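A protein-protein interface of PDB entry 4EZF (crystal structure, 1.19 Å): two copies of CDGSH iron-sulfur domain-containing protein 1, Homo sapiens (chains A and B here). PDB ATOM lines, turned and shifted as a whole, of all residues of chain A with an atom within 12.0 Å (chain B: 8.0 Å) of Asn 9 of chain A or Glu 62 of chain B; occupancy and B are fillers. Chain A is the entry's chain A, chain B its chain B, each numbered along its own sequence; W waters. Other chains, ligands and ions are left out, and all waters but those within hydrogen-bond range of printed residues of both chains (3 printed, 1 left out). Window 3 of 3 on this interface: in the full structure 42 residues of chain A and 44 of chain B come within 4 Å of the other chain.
Water W3 lies within hydrogen-bond range of the backbone carbonyl oxygen (O) of Gly 64 of chain B (2.7 Å) and the side-chain amino group (NZ) of Lys 19 of chain A (2.8 Å).
Water W1 bridges the backbone carbonyl oxygen of Ala 11 of chain B and the guanidinium group of Arg 45 of chain A.
Water W2 lies within hydrogen-bond range of O of Ala 11 of chain A (2.9 Å) and NH2 of Arg 45 of chain B (2.9 Å).
Positions printed for both chains: 11 and 45.
The side-chain amide oxygen (OD1) of Asn 9 of chain A lies within hydrogen-bond range of the backbone NH (N) of Ala 11 of chain A.
O of Ile 13 of chain A lies within hydrogen-bond range of NH1 of Arg 45 of chain A (2.7 Å).
O of Asn 14 of chain A lies within hydrogen-bond range of NZ of Lys 19 of chain A (2.8 Å).
The side-chain carboxylate (OE1) of Glu 62 of chain B lies within salt-bridge range of the side-chain amino group (NZ) of Lys 58 of chain B, at 3.0 Å.
The backbone carbonyl oxygen (O) of His 59 of chain B lies within hydrogen-bond range of the side-chain hydroxyl (OG1) of Thr 63 of chain B, 2.9 Å away.
The backbone NH (N) of Asp 65 of chain B sits close to the side-chain hydroxyl (OG1) of Thr 63 of chain B, at 3.4 Å.
Asn 9 of chain A touches just these residues of chain B: Glu 62 (3.3 Å) and Thr 63 (3.4 Å).
Glu 62 of chain B touches one residue of chain A.
Arg 8 of chain A touches none of the printed residues of chain B.
No residue of chain A comes within 4 Å of Lys 58 of chain B.
Of chain A, only Ala 11 and Ile 13 come within 4 Å of His 59 of chain B.
Glu 61 of chain B touches none of the printed residues of chain A.
Gly 64 of chain B touches none of the printed residues of chain A.
Of the printed residues of chain B, Lys 19 of chain A touches Asp 65.
Of the printed residues of chain B, Asn 14 of chain A touches Asp 65 (3.1 Å).
Printed residues of chain B within 4 Å of Met 12 of chain A: Asp 65.
Printed residues of chain A within 4 Å of Arg 45 of chain B: Ile 13 (3.9 Å).
Of the printed residues of chain B, Ile 13 of chain A touches Arg 45, His 59 and Asp 65.
Asn 60 of chain B touches none of the printed residues of chain A.
The nearest residue of chain B that does not touch Asn 9 of chain A is Gly 64 of chain B (5.2 Å).
Printed residues of chain B that touch a printed residue of chain A: Ala 11, Arg 45, His 59, Glu 62, Thr 63 and Asp 65.
Printed residues of chain A that touch a printed residue of chain B: Asn 9, Lys 10, Ala 11, Met 12, Ile 13, Asn 14 and Lys 19.
Hydrophobic or aromatic side chains of chain A that line the printed part of chain B: Ala 11, Met 12 and Ile 13.
Among the printed residues, Asp or Glu carboxylates within 4 Å of a Lys or Arg side-chain nitrogen of the other chain: Lys 19 of chain A with Asp 65 of chain B (3.0 Å).
The side-chain amide nitrogen of Asn 9 of chain A sits at hydrogen-bond distance from the backbone carbonyl oxygen of Glu 62 of chain B, at 3.3 Å.
OD2 of Asp 65 of chain B sits at hydrogen-bond distance from N of Ile 13 of chain A (2.8 Å).
The backbone NH (N) of Asn 14 of chain A lies within hydrogen-bond range of the side-chain carboxylate (OD2) of Asp 65 of chain B (3.1 Å).
The side-chain carboxylate (OD1) of Asp 65 of chain B lies within salt-bridge range of the side-chain amino group (NZ) of Lys 19 of chain A.
Among the printed residues, merely in contact across the chains: Asn 9 of chain A with Thr 63 of chain B, Lys 10 of chain A with Ala 11 of chain B, Ala 11 of chain A with His 59 of chain B, Ala 11 of chain A with Thr 63 of chain B, Met 12 of chain A with Asp 65 of chain B, Ile 13 of chain A with Arg 45 of chain B and Ile 13 of chain A with His 59 of chain B.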
ATOM      1  N   LYS A   5     -33.110  -8.096 -13.713  1.00  0.00           N
ATOM      2  CA  LYS A   5     -32.460  -6.801 -13.730  1.00  0.00           C
ATOM      3  C   LYS A   5     -31.027  -7.022 -13.275  1.00  0.00           C
ATOM      4  O   LYS A   5     -30.760  -7.872 -12.421  1.00  0.00           O
ATOM      5  CB  LYS A   5     -33.201  -5.820 -12.822  1.00  0.00           C
ATOM      6  CG  LYS A   5     -34.704  -5.838 -13.062  1.00  0.00           C
ATOM      7  CD  LYS A   5     -35.367  -4.525 -12.729  1.00  0.00           C
ATOM      8  CE  LYS A   5     -36.832  -4.559 -13.129  1.00  0.00           C
ATOM      9  NZ  LYS A   5     -37.555  -3.346 -12.653  1.00  0.00           N
ATOM     10  N   ASP A   6     -30.102  -6.295 -13.889  1.00  0.00           N
ATOM     11  CA  ASP A   6     -28.698  -6.354 -13.515  1.00  0.00           C
ATOM     12  C   ASP A   6     -28.286  -4.933 -13.182  1.00  0.00           C
ATOM     13  O   ASP A   6     -28.297  -4.058 -14.054  1.00  0.00           O
ATOM     14  CB  ASP A   6     -27.851  -6.897 -14.671  1.00  0.00           C
ATOM     15  N   HIS A   7     -27.946  -4.695 -11.920  1.00  0.00           N
ATOM     16  CA  HIS A   7     -27.657  -3.338 -11.472  1.00  0.00           C
ATOM     17  C   HIS A   7     -26.173  -2.994 -11.522  1.00  0.00           C
ATOM     18  O   HIS A   7     -25.757  -1.961 -11.005  1.00  0.00           O
ATOM     19  CB  HIS A   7     -28.224  -3.106 -10.072  1.00  0.00           C
ATOM     20  CG  HIS A   7     -29.705  -3.310  -9.983  1.00  0.00           C
ATOM     21  ND1 HIS A   7     -30.600  -2.644 -10.794  1.00  0.00           N
ATOM     22  CD2 HIS A   7     -30.451  -4.095  -9.167  1.00  0.00           C
ATOM     23  CE1 HIS A   7     -31.831  -3.011 -10.483  1.00  0.00           C
ATOM     24  NE2 HIS A   7     -31.767  -3.900  -9.507  1.00  0.00           N
ATOM     25  N   ARG A   8     -25.383  -3.852 -12.164  1.00  0.00           N
ATOM     26  CA  ARG A   8     -23.976  -3.549 -12.419  1.00  0.00           C
ATOM     27  C   ARG A   8     -23.867  -2.389 -13.409  1.00  0.00           C
ATOM     28  O   ARG A   8     -24.822  -2.085 -14.121  1.00  0.00           O
ATOM     29  CB  ARG A   8     -23.246  -4.780 -12.961  1.00  0.00           C
ATOM     30  N   ASN A   9     -22.709  -1.735 -13.439  1.00  0.00           N
ATOM     31  CA  ASN A   9     -22.498  -0.613 -14.341  1.00  0.00           C
ATOM     32  C   ASN A   9     -22.639  -1.084 -15.779  1.00  0.00           C
ATOM     33  O   ASN A   9     -21.978  -2.037 -16.190  1.00  0.00           O
ATOM     34  CB  ASN A   9     -21.115  -0.002 -14.114  1.00  0.00           C
ATOM     35  CG  ASN A   9     -20.930   1.321 -14.841  1.00  0.00           C
ATOM     36  OD1 ASN A   9     -20.909   1.373 -16.075  1.00  0.00           O
ATOM     37  ND2 ASN A   9     -20.772   2.400 -14.076  1.00  0.00           N
ATOM     38  N   LYS A  10     -23.509  -0.426 -16.540  1.00  0.00           N
ATOM     39  CA  LYS A  10     -23.787  -0.841 -17.911  1.00  0.00           C
ATOM     40  C   LYS A  10     -22.560  -0.732 -18.823  1.00  0.00           C
ATOM     41  O   LYS A  10     -22.521  -1.330 -19.893  1.00  0.00           O
ATOM     42  CB  LYS A  10     -24.957  -0.034 -18.491  1.00  0.00           C
ATOM     43  N   ALA A  11     -21.559   0.032 -18.396  1.00  0.00           N
ATOM     44  CA  ALA A  11     -20.375   0.235 -19.214  1.00  0.00           C
ATOM     45  C   ALA A  11     -19.277  -0.798 -18.988  1.00  0.00           C
ATOM     46  O   ALA A  11     -18.284  -0.765 -19.702  1.00  0.00           O
ATOM     47  CB  ALA A  11     -19.826   1.638 -19.035  1.00  0.00           C
ATOM     48  N   MET A  12     -19.468  -1.718 -18.037  1.00  0.00           N
ATOM     49  CA  MET A  12     -18.510  -2.819 -17.806  1.00  0.00           C
ATOM     50  C   MET A  12     -18.220  -3.594 -19.117  1.00  0.00           C
ATOM     51  O   MET A  12     -19.140  -3.864 -19.888  1.00  0.00           O
ATOM     52  CB  MET A  12     -19.046  -3.762 -16.718  1.00  0.00           C
ATOM     53  CG  MET A  12     -18.037  -4.811 -16.235  1.00  0.00           C
ATOM     54  SD  MET A  12     -18.246  -5.426 -14.513  1.00  0.00           S
ATOM     55  CE  MET A  12     -19.141  -6.948 -14.772  1.00  0.00           C
ATOM     56  N   ILE A  13     -16.948  -3.906 -19.369  1.00  0.00           N
ATOM     57  CA  ILE A  13     -16.510  -4.601 -20.583  1.00  0.00           C
ATOM     58  C   ILE A  13     -16.453  -6.098 -20.365  1.00  0.00           C
ATOM     59  O   ILE A  13     -17.033  -6.858 -21.152  1.00  0.00           O
ATOM     60  CB  ILE A  13     -15.157  -4.049 -21.054  1.00  0.00           C
ATOM     61  CG1 ILE A  13     -15.361  -2.625 -21.578  1.00  0.00           C
ATOM     62  CG2 ILE A  13     -14.496  -4.963 -22.091  1.00  0.00           C
ATOM     63  CD1 ILE A  13     -14.080  -1.898 -21.826  1.00  0.00           C
ATOM     64  N   ASN A  14     -15.758  -6.535 -19.305  1.00  0.00           N
ATOM     65  CA  ASN A  14     -15.687  -7.948 -18.996  1.00  0.00           C
ATOM     66  C   ASN A  14     -16.826  -8.325 -18.064  1.00  0.00           C
ATOM     67  O   ASN A  14     -16.922  -7.798 -16.959  1.00  0.00           O
ATOM     68  CB  ASN A  14     -14.331  -8.259 -18.364  1.00  0.00           C
ATOM     69  CG  ASN A  14     -14.248  -9.674 -17.853  1.00  0.00           C
ATOM     70  OD1 ASN A  14     -14.889 -10.590 -18.375  1.00  0.00           O
ATOM     71  ND2 ASN A  14     -13.461  -9.866 -16.797  1.00  0.00           N
ATOM     72  N   LEU A  15     -17.697  -9.217 -18.518  1.00  0.00           N
ATOM     73  CA  LEU A  15     -18.869  -9.585 -17.740  1.00  0.00           C
ATOM     74  C   LEU A  15     -18.603 -10.745 -16.785  1.00  0.00           C
ATOM     75  O   LEU A  15     -19.149 -10.774 -15.678  1.00  0.00           O
ATOM     76  CB  LEU A  15     -20.024  -9.935 -18.680  1.00  0.00           C
ATOM     77  CG  LEU A  15     -20.414  -8.802 -19.627  1.00  0.00           C
ATOM     78  CD1 LEU A  15     -21.526  -9.221 -20.603  1.00  0.00           C
ATOM     79  CD2 LEU A  15     -20.823  -7.595 -18.807  1.00  0.00           C
ATOM     80  N   HIS A  16     -17.760 -11.690 -17.191  1.00  0.00           N
ATOM     81  CA  HIS A  16     -17.715 -12.982 -16.512  1.00  0.00           C
ATOM     82  C   HIS A  16     -16.331 -13.565 -16.252  1.00  0.00           C
ATOM     83  O   HIS A  16     -16.211 -14.517 -15.491  1.00  0.00           O
ATOM     84  CB  HIS A  16     -18.541 -14.010 -17.305  1.00  0.00           C
ATOM     85  CG  HIS A  16     -19.981 -13.637 -17.461  1.00  0.00           C
ATOM     86  ND1 HIS A  16     -20.577 -13.454 -18.689  1.00  0.00           N
ATOM     87  CD2 HIS A  16     -20.945 -13.406 -16.536  1.00  0.00           C
ATOM     88  CE1 HIS A  16     -21.846 -13.125 -18.516  1.00  0.00           C
ATOM     89  NE2 HIS A  16     -22.095 -13.094 -17.220  1.00  0.00           N
ATOM     90  N   LYS A  19     -13.285 -13.091 -12.216  1.00  0.00           N
ATOM     91  CA  LYS A  19     -13.644 -11.899 -11.475  1.00  0.00           C
ATOM     92  C   LYS A  19     -12.976 -11.809 -10.084  1.00  0.00           C
ATOM     93  O   LYS A  19     -13.074 -10.771  -9.447  1.00  0.00           O
ATOM     94  CB  LYS A  19     -15.164 -11.762 -11.389  1.00  0.00           C
ATOM     95  CG  LYS A  19     -15.793 -11.332 -12.719  1.00  0.00           C
ATOM     96  CD  LYS A  19     -15.360  -9.914 -13.035  1.00  0.00           C
ATOM     97  CE  LYS A  19     -15.998  -9.377 -14.317  1.00  0.00           C
ATOM     98  NZ  LYS A  19     -15.521  -8.000 -14.586  1.00  0.00           N
ATOM     99  N   PRO A  22      -8.274  -8.818  -9.668  1.00  0.00           N
ATOM    100  CA  PRO A  22      -8.678  -7.409  -9.748  1.00  0.00           C
ATOM    101  C   PRO A  22      -8.218  -6.700 -11.030  1.00  0.00           C
ATOM    102  O   PRO A  22      -8.736  -5.626 -11.319  1.00  0.00           O
ATOM    103  CB  PRO A  22      -8.021  -6.772  -8.528  1.00  0.00           C
ATOM    104  CG  PRO A  22      -6.922  -7.700  -8.159  1.00  0.00           C
ATOM    105  CD  PRO A  22      -7.305  -9.066  -8.579  1.00  0.00           C
ATOM    106  N   ARG A  45     -15.285 -11.904 -24.626  1.00  0.00           N
ATOM    107  CA  ARG A  45     -16.384 -12.849 -24.783  1.00  0.00           C
ATOM    108  C   ARG A  45     -15.935 -14.249 -25.181  1.00  0.00           C
ATOM    109  O   ARG A  45     -16.743 -15.190 -25.177  1.00  0.00           O
ATOM    110  CB  ARG A  45     -17.424 -12.327 -25.774  1.00  0.00           C
ATOM    111  CG  ARG A  45     -17.986 -10.946 -25.422  1.00  0.00           C
ATOM    112  CD  ARG A  45     -18.977 -10.971 -24.268  1.00  0.00           C
ATOM    113  NE  ARG A  45     -19.464  -9.624 -23.979  1.00  0.00           N
ATOM    114  CZ  ARG A  45     -18.839  -8.749 -23.201  1.00  0.00           C
ATOM    115  NH1 ARG A  45     -17.721  -9.101 -22.561  1.00  0.00           N
ATOM    116  NH2 ARG A  45     -19.356  -7.530 -23.013  1.00  0.00           N
ATOM    117  N   ALA B  11     -24.357  -3.616 -23.946  1.00  0.00           N
ATOM    118  CA  ALA B  11     -23.549  -2.442 -24.246  1.00  0.00           C
ATOM    119  C   ALA B  11     -22.427  -2.766 -25.228  1.00  0.00           C
ATOM    120  O   ALA B  11     -21.918  -3.894 -25.261  1.00  0.00           O
ATOM    121  CB  ALA B  11     -22.969  -1.870 -22.969  1.00  0.00           C
ATOM    122  N   ARG B  45     -10.153   1.996 -24.404  1.00  0.00           N
ATOM    123  CA  ARG B  45     -10.210   3.359 -23.869  1.00  0.00           C
ATOM    124  C   ARG B  45      -8.886   4.109 -24.058  1.00  0.00           C
ATOM    125  O   ARG B  45      -8.818   5.308 -23.804  1.00  0.00           O
ATOM    126  CB  ARG B  45     -10.563   3.359 -22.373  1.00  0.00           C
ATOM    127  CG  ARG B  45     -11.877   2.697 -22.026  1.00  0.00           C
ATOM    128  CD  ARG B  45     -13.055   3.505 -22.566  1.00  0.00           C
ATOM    129  NE  ARG B  45     -14.313   2.860 -22.235  1.00  0.00           N
ATOM    130  CZ  ARG B  45     -14.910   1.938 -22.987  1.00  0.00           C
ATOM    131  NH1 ARG B  45     -14.405   1.574 -24.160  1.00  0.00           N
ATOM    132  NH2 ARG B  45     -16.040   1.390 -22.578  1.00  0.00           N
ATOM    133  N   ALA B  55      -5.304   3.797 -19.511  1.00  0.00           N
ATOM    134  CA  ALA B  55      -6.707   4.172 -19.398  1.00  0.00           C
ATOM    135  C   ALA B  55      -7.570   3.084 -18.740  1.00  0.00           C
ATOM    136  O   ALA B  55      -8.630   3.381 -18.189  1.00  0.00           O
ATOM    137  CB  ALA B  55      -7.272   4.582 -20.775  1.00  0.00           C
ATOM    138  N   HIS B  56      -7.119   1.825 -18.799  1.00  0.00           N
ATOM    139  CA  HIS B  56      -7.870   0.731 -18.173  1.00  0.00           C
ATOM    140  C   HIS B  56      -8.085   0.974 -16.675  1.00  0.00           C
ATOM    141  O   HIS B  56      -9.104   0.554 -16.128  1.00  0.00           O
ATOM    142  CB  HIS B  56      -7.207  -0.630 -18.392  1.00  0.00           C
ATOM    143  CG  HIS B  56      -5.813  -0.717 -17.866  1.00  0.00           C
ATOM    144  ND1 HIS B  56      -4.695  -0.451 -18.635  1.00  0.00           N
ATOM    145  CD2 HIS B  56      -5.355  -1.031 -16.630  1.00  0.00           C
ATOM    146  CE1 HIS B  56      -3.610  -0.592 -17.882  1.00  0.00           C
ATOM    147  NE2 HIS B  56      -3.982  -0.959 -16.672  1.00  0.00           N
ATOM    148  N   THR B  57      -7.159   1.660 -15.996  1.00  0.00           N
ATOM    149  CA  THR B  57      -7.335   1.845 -14.545  1.00  0.00           C
ATOM    150  C   THR B  57      -8.534   2.745 -14.249  1.00  0.00           C
ATOM    151  O   THR B  57      -9.324   2.480 -13.321  1.00  0.00           O
ATOM    152  CB  THR B  57      -6.067   2.367 -13.851  1.00  0.00           C
ATOM    153  OG1 THR B  57      -5.762   3.667 -14.344  1.00  0.00           O
ATOM    154  CG2 THR B  57      -4.900   1.448 -14.086  1.00  0.00           C
ATOM    155  N   LYS B  58      -8.699   3.787 -15.059  1.00  0.00           N
ATOM    156  CA  LYS B  58      -9.832   4.688 -14.889  1.00  0.00           C
ATOM    157  C   LYS B  58     -11.129   3.961 -15.241  1.00  0.00           C
ATOM    158  O   LYS B  58     -12.134   4.075 -14.547  1.00  0.00           O
ATOM    159  CB  LYS B  58      -9.663   5.915 -15.777  1.00  0.00           C
ATOM    160  CG  LYS B  58     -10.846   6.883 -15.744  1.00  0.00           C
ATOM    161  CD  LYS B  58     -10.608   8.103 -16.641  1.00  0.00           C
ATOM    162  CE  LYS B  58     -11.726   9.140 -16.538  1.00  0.00           C
ATOM    163  NZ  LYS B  58     -12.883   8.831 -17.431  1.00  0.00           N
ATOM    164  N   HIS B  59     -11.101   3.201 -16.332  1.00  0.00           N
ATOM    165  CA  HIS B  59     -12.255   2.388 -16.677  1.00  0.00           C
ATOM    166  C   HIS B  59     -12.664   1.441 -15.555  1.00  0.00           C
ATOM    167  O   HIS B  59     -13.838   1.371 -15.207  1.00  0.00           O
ATOM    168  CB  HIS B  59     -12.025   1.592 -17.978  1.00  0.00           C
ATOM    169  CG  HIS B  59     -13.027   0.500 -18.181  1.00  0.00           C
ATOM    170  ND1 HIS B  59     -14.280   0.722 -18.712  1.00  0.00           N
ATOM    171  CD2 HIS B  59     -12.964  -0.825 -17.901  1.00  0.00           C
ATOM    172  CE1 HIS B  59     -14.953  -0.416 -18.722  1.00  0.00           C
ATOM    173  NE2 HIS B  59     -14.177  -1.369 -18.229  1.00  0.00           N
ATOM    174  N   ASN B  60     -11.700   0.707 -15.006  1.00  0.00           N
ATOM    175  CA  ASN B  60     -11.981  -0.265 -13.943  1.00  0.00           C
ATOM    176  C   ASN B  60     -12.581   0.391 -12.702  1.00  0.00           C
ATOM    177  O   ASN B  60     -13.511  -0.131 -12.107  1.00  0.00           O
ATOM    178  CB  ASN B  60     -10.705  -1.027 -13.567  1.00  0.00           C
ATOM    179  CG  ASN B  60     -10.301  -2.048 -14.633  1.00  0.00           C
ATOM    180  OD1 ASN B  60     -11.124  -2.477 -15.469  1.00  0.00           O
ATOM    181  ND2 ASN B  60      -9.051  -2.458 -14.606  1.00  0.00           N
ATOM    182  N   GLU B  61     -12.061   1.550 -12.328  1.00  0.00           N
ATOM    183  CA  GLU B  61     -12.632   2.299 -11.210  1.00  0.00           C
ATOM    184  C   GLU B  61     -14.033   2.858 -11.500  1.00  0.00           C
ATOM    185  O   GLU B  61     -14.912   2.838 -10.625  1.00  0.00           O
ATOM    186  CB  GLU B  61     -11.685   3.420 -10.826  1.00  0.00           C
ATOM    187  CG  GLU B  61     -12.136   4.195  -9.612  1.00  0.00           C
ATOM    188  CD  GLU B  61     -11.110   5.211  -9.187  1.00  0.00           C
ATOM    189  OE1 GLU B  61     -10.797   6.113  -9.998  1.00  0.00           O
ATOM    190  OE2 GLU B  61     -10.621   5.096  -8.047  1.00  0.00           O
ATOM    191  N   GLU B  62     -14.240   3.393 -12.701  1.00  0.00           N
ATOM    192  CA  GLU B  62     -15.532   3.990 -13.056  1.00  0.00           C
ATOM    193  C   GLU B  62     -16.655   2.956 -13.158  1.00  0.00           C
ATOM    194  O   GLU B  62     -17.822   3.265 -12.889  1.00  0.00           O
ATOM    195  CB  GLU B  62     -15.428   4.735 -14.390  1.00  0.00           C
ATOM    196  CG  GLU B  62     -14.776   6.096 -14.300  1.00  0.00           C
ATOM    197  CD  GLU B  62     -14.972   6.895 -15.571  1.00  0.00           C
ATOM    198  OE1 GLU B  62     -14.554   6.415 -16.643  1.00  0.00           O
ATOM    199  OE2 GLU B  62     -15.565   7.994 -15.512  1.00  0.00           O
ATOM    200  N   THR B  63     -16.317   1.734 -13.558  1.00  0.00           N
ATOM    201  CA  THR B  63     -17.336   0.743 -13.886  1.00  0.00           C
ATOM    202  C   THR B  63     -17.297  -0.501 -13.002  1.00  0.00           C
ATOM    203  O   THR B  63     -18.165  -1.371 -13.116  1.00  0.00           O
ATOM    204  CB  THR B  63     -17.192   0.262 -15.345  1.00  0.00           C
ATOM    205  OG1 THR B  63     -16.005  -0.532 -15.472  1.00  0.00           O
ATOM    206  CG2 THR B  63     -17.139   1.452 -16.313  1.00  0.00           C
ATOM    207  N   GLY B  64     -16.294  -0.609 -12.136  1.00  0.00           N
ATOM    208  CA  GLY B  64     -16.132  -1.803 -11.322  1.00  0.00           C
ATOM    209  C   GLY B  64     -15.509  -3.006 -12.032  1.00  0.00           C
ATOM    210  O   GLY B  64     -15.521  -4.121 -11.529  1.00  0.00           O
ATOM    211  N   ASP B  65     -14.940  -2.782 -13.208  1.00  0.00           N
ATOM    212  CA  ASP B  65     -14.397  -3.852 -14.037  1.00  0.00           C
ATOM    213  C   ASP B  65     -12.989  -4.246 -13.593  1.00  0.00           C
ATOM    214  O   ASP B  65     -12.434  -3.668 -12.652  1.00  0.00           O
ATOM    215  CB  ASP B  65     -14.360  -3.351 -15.472  1.00  0.00           C
ATOM    216  CG  ASP B  65     -14.550  -4.450 -16.518  1.00  0.00           C
ATOM    217  OD1 ASP B  65     -14.505  -5.663 -16.193  1.00  0.00           O
ATOM    218  OD2 ASP B  65     -14.751  -4.057 -17.689  1.00  0.00           O
HETATM  219  O   HOH W   1     -21.835  -6.266 -23.901  1.00  0.00           O
HETATM  220  O   HOH W   2     -18.516  -0.100 -22.482  1.00  0.00           O
HETATM  221  O   HOH W   3     -15.300  -6.760 -12.121  1.00  0.00           O
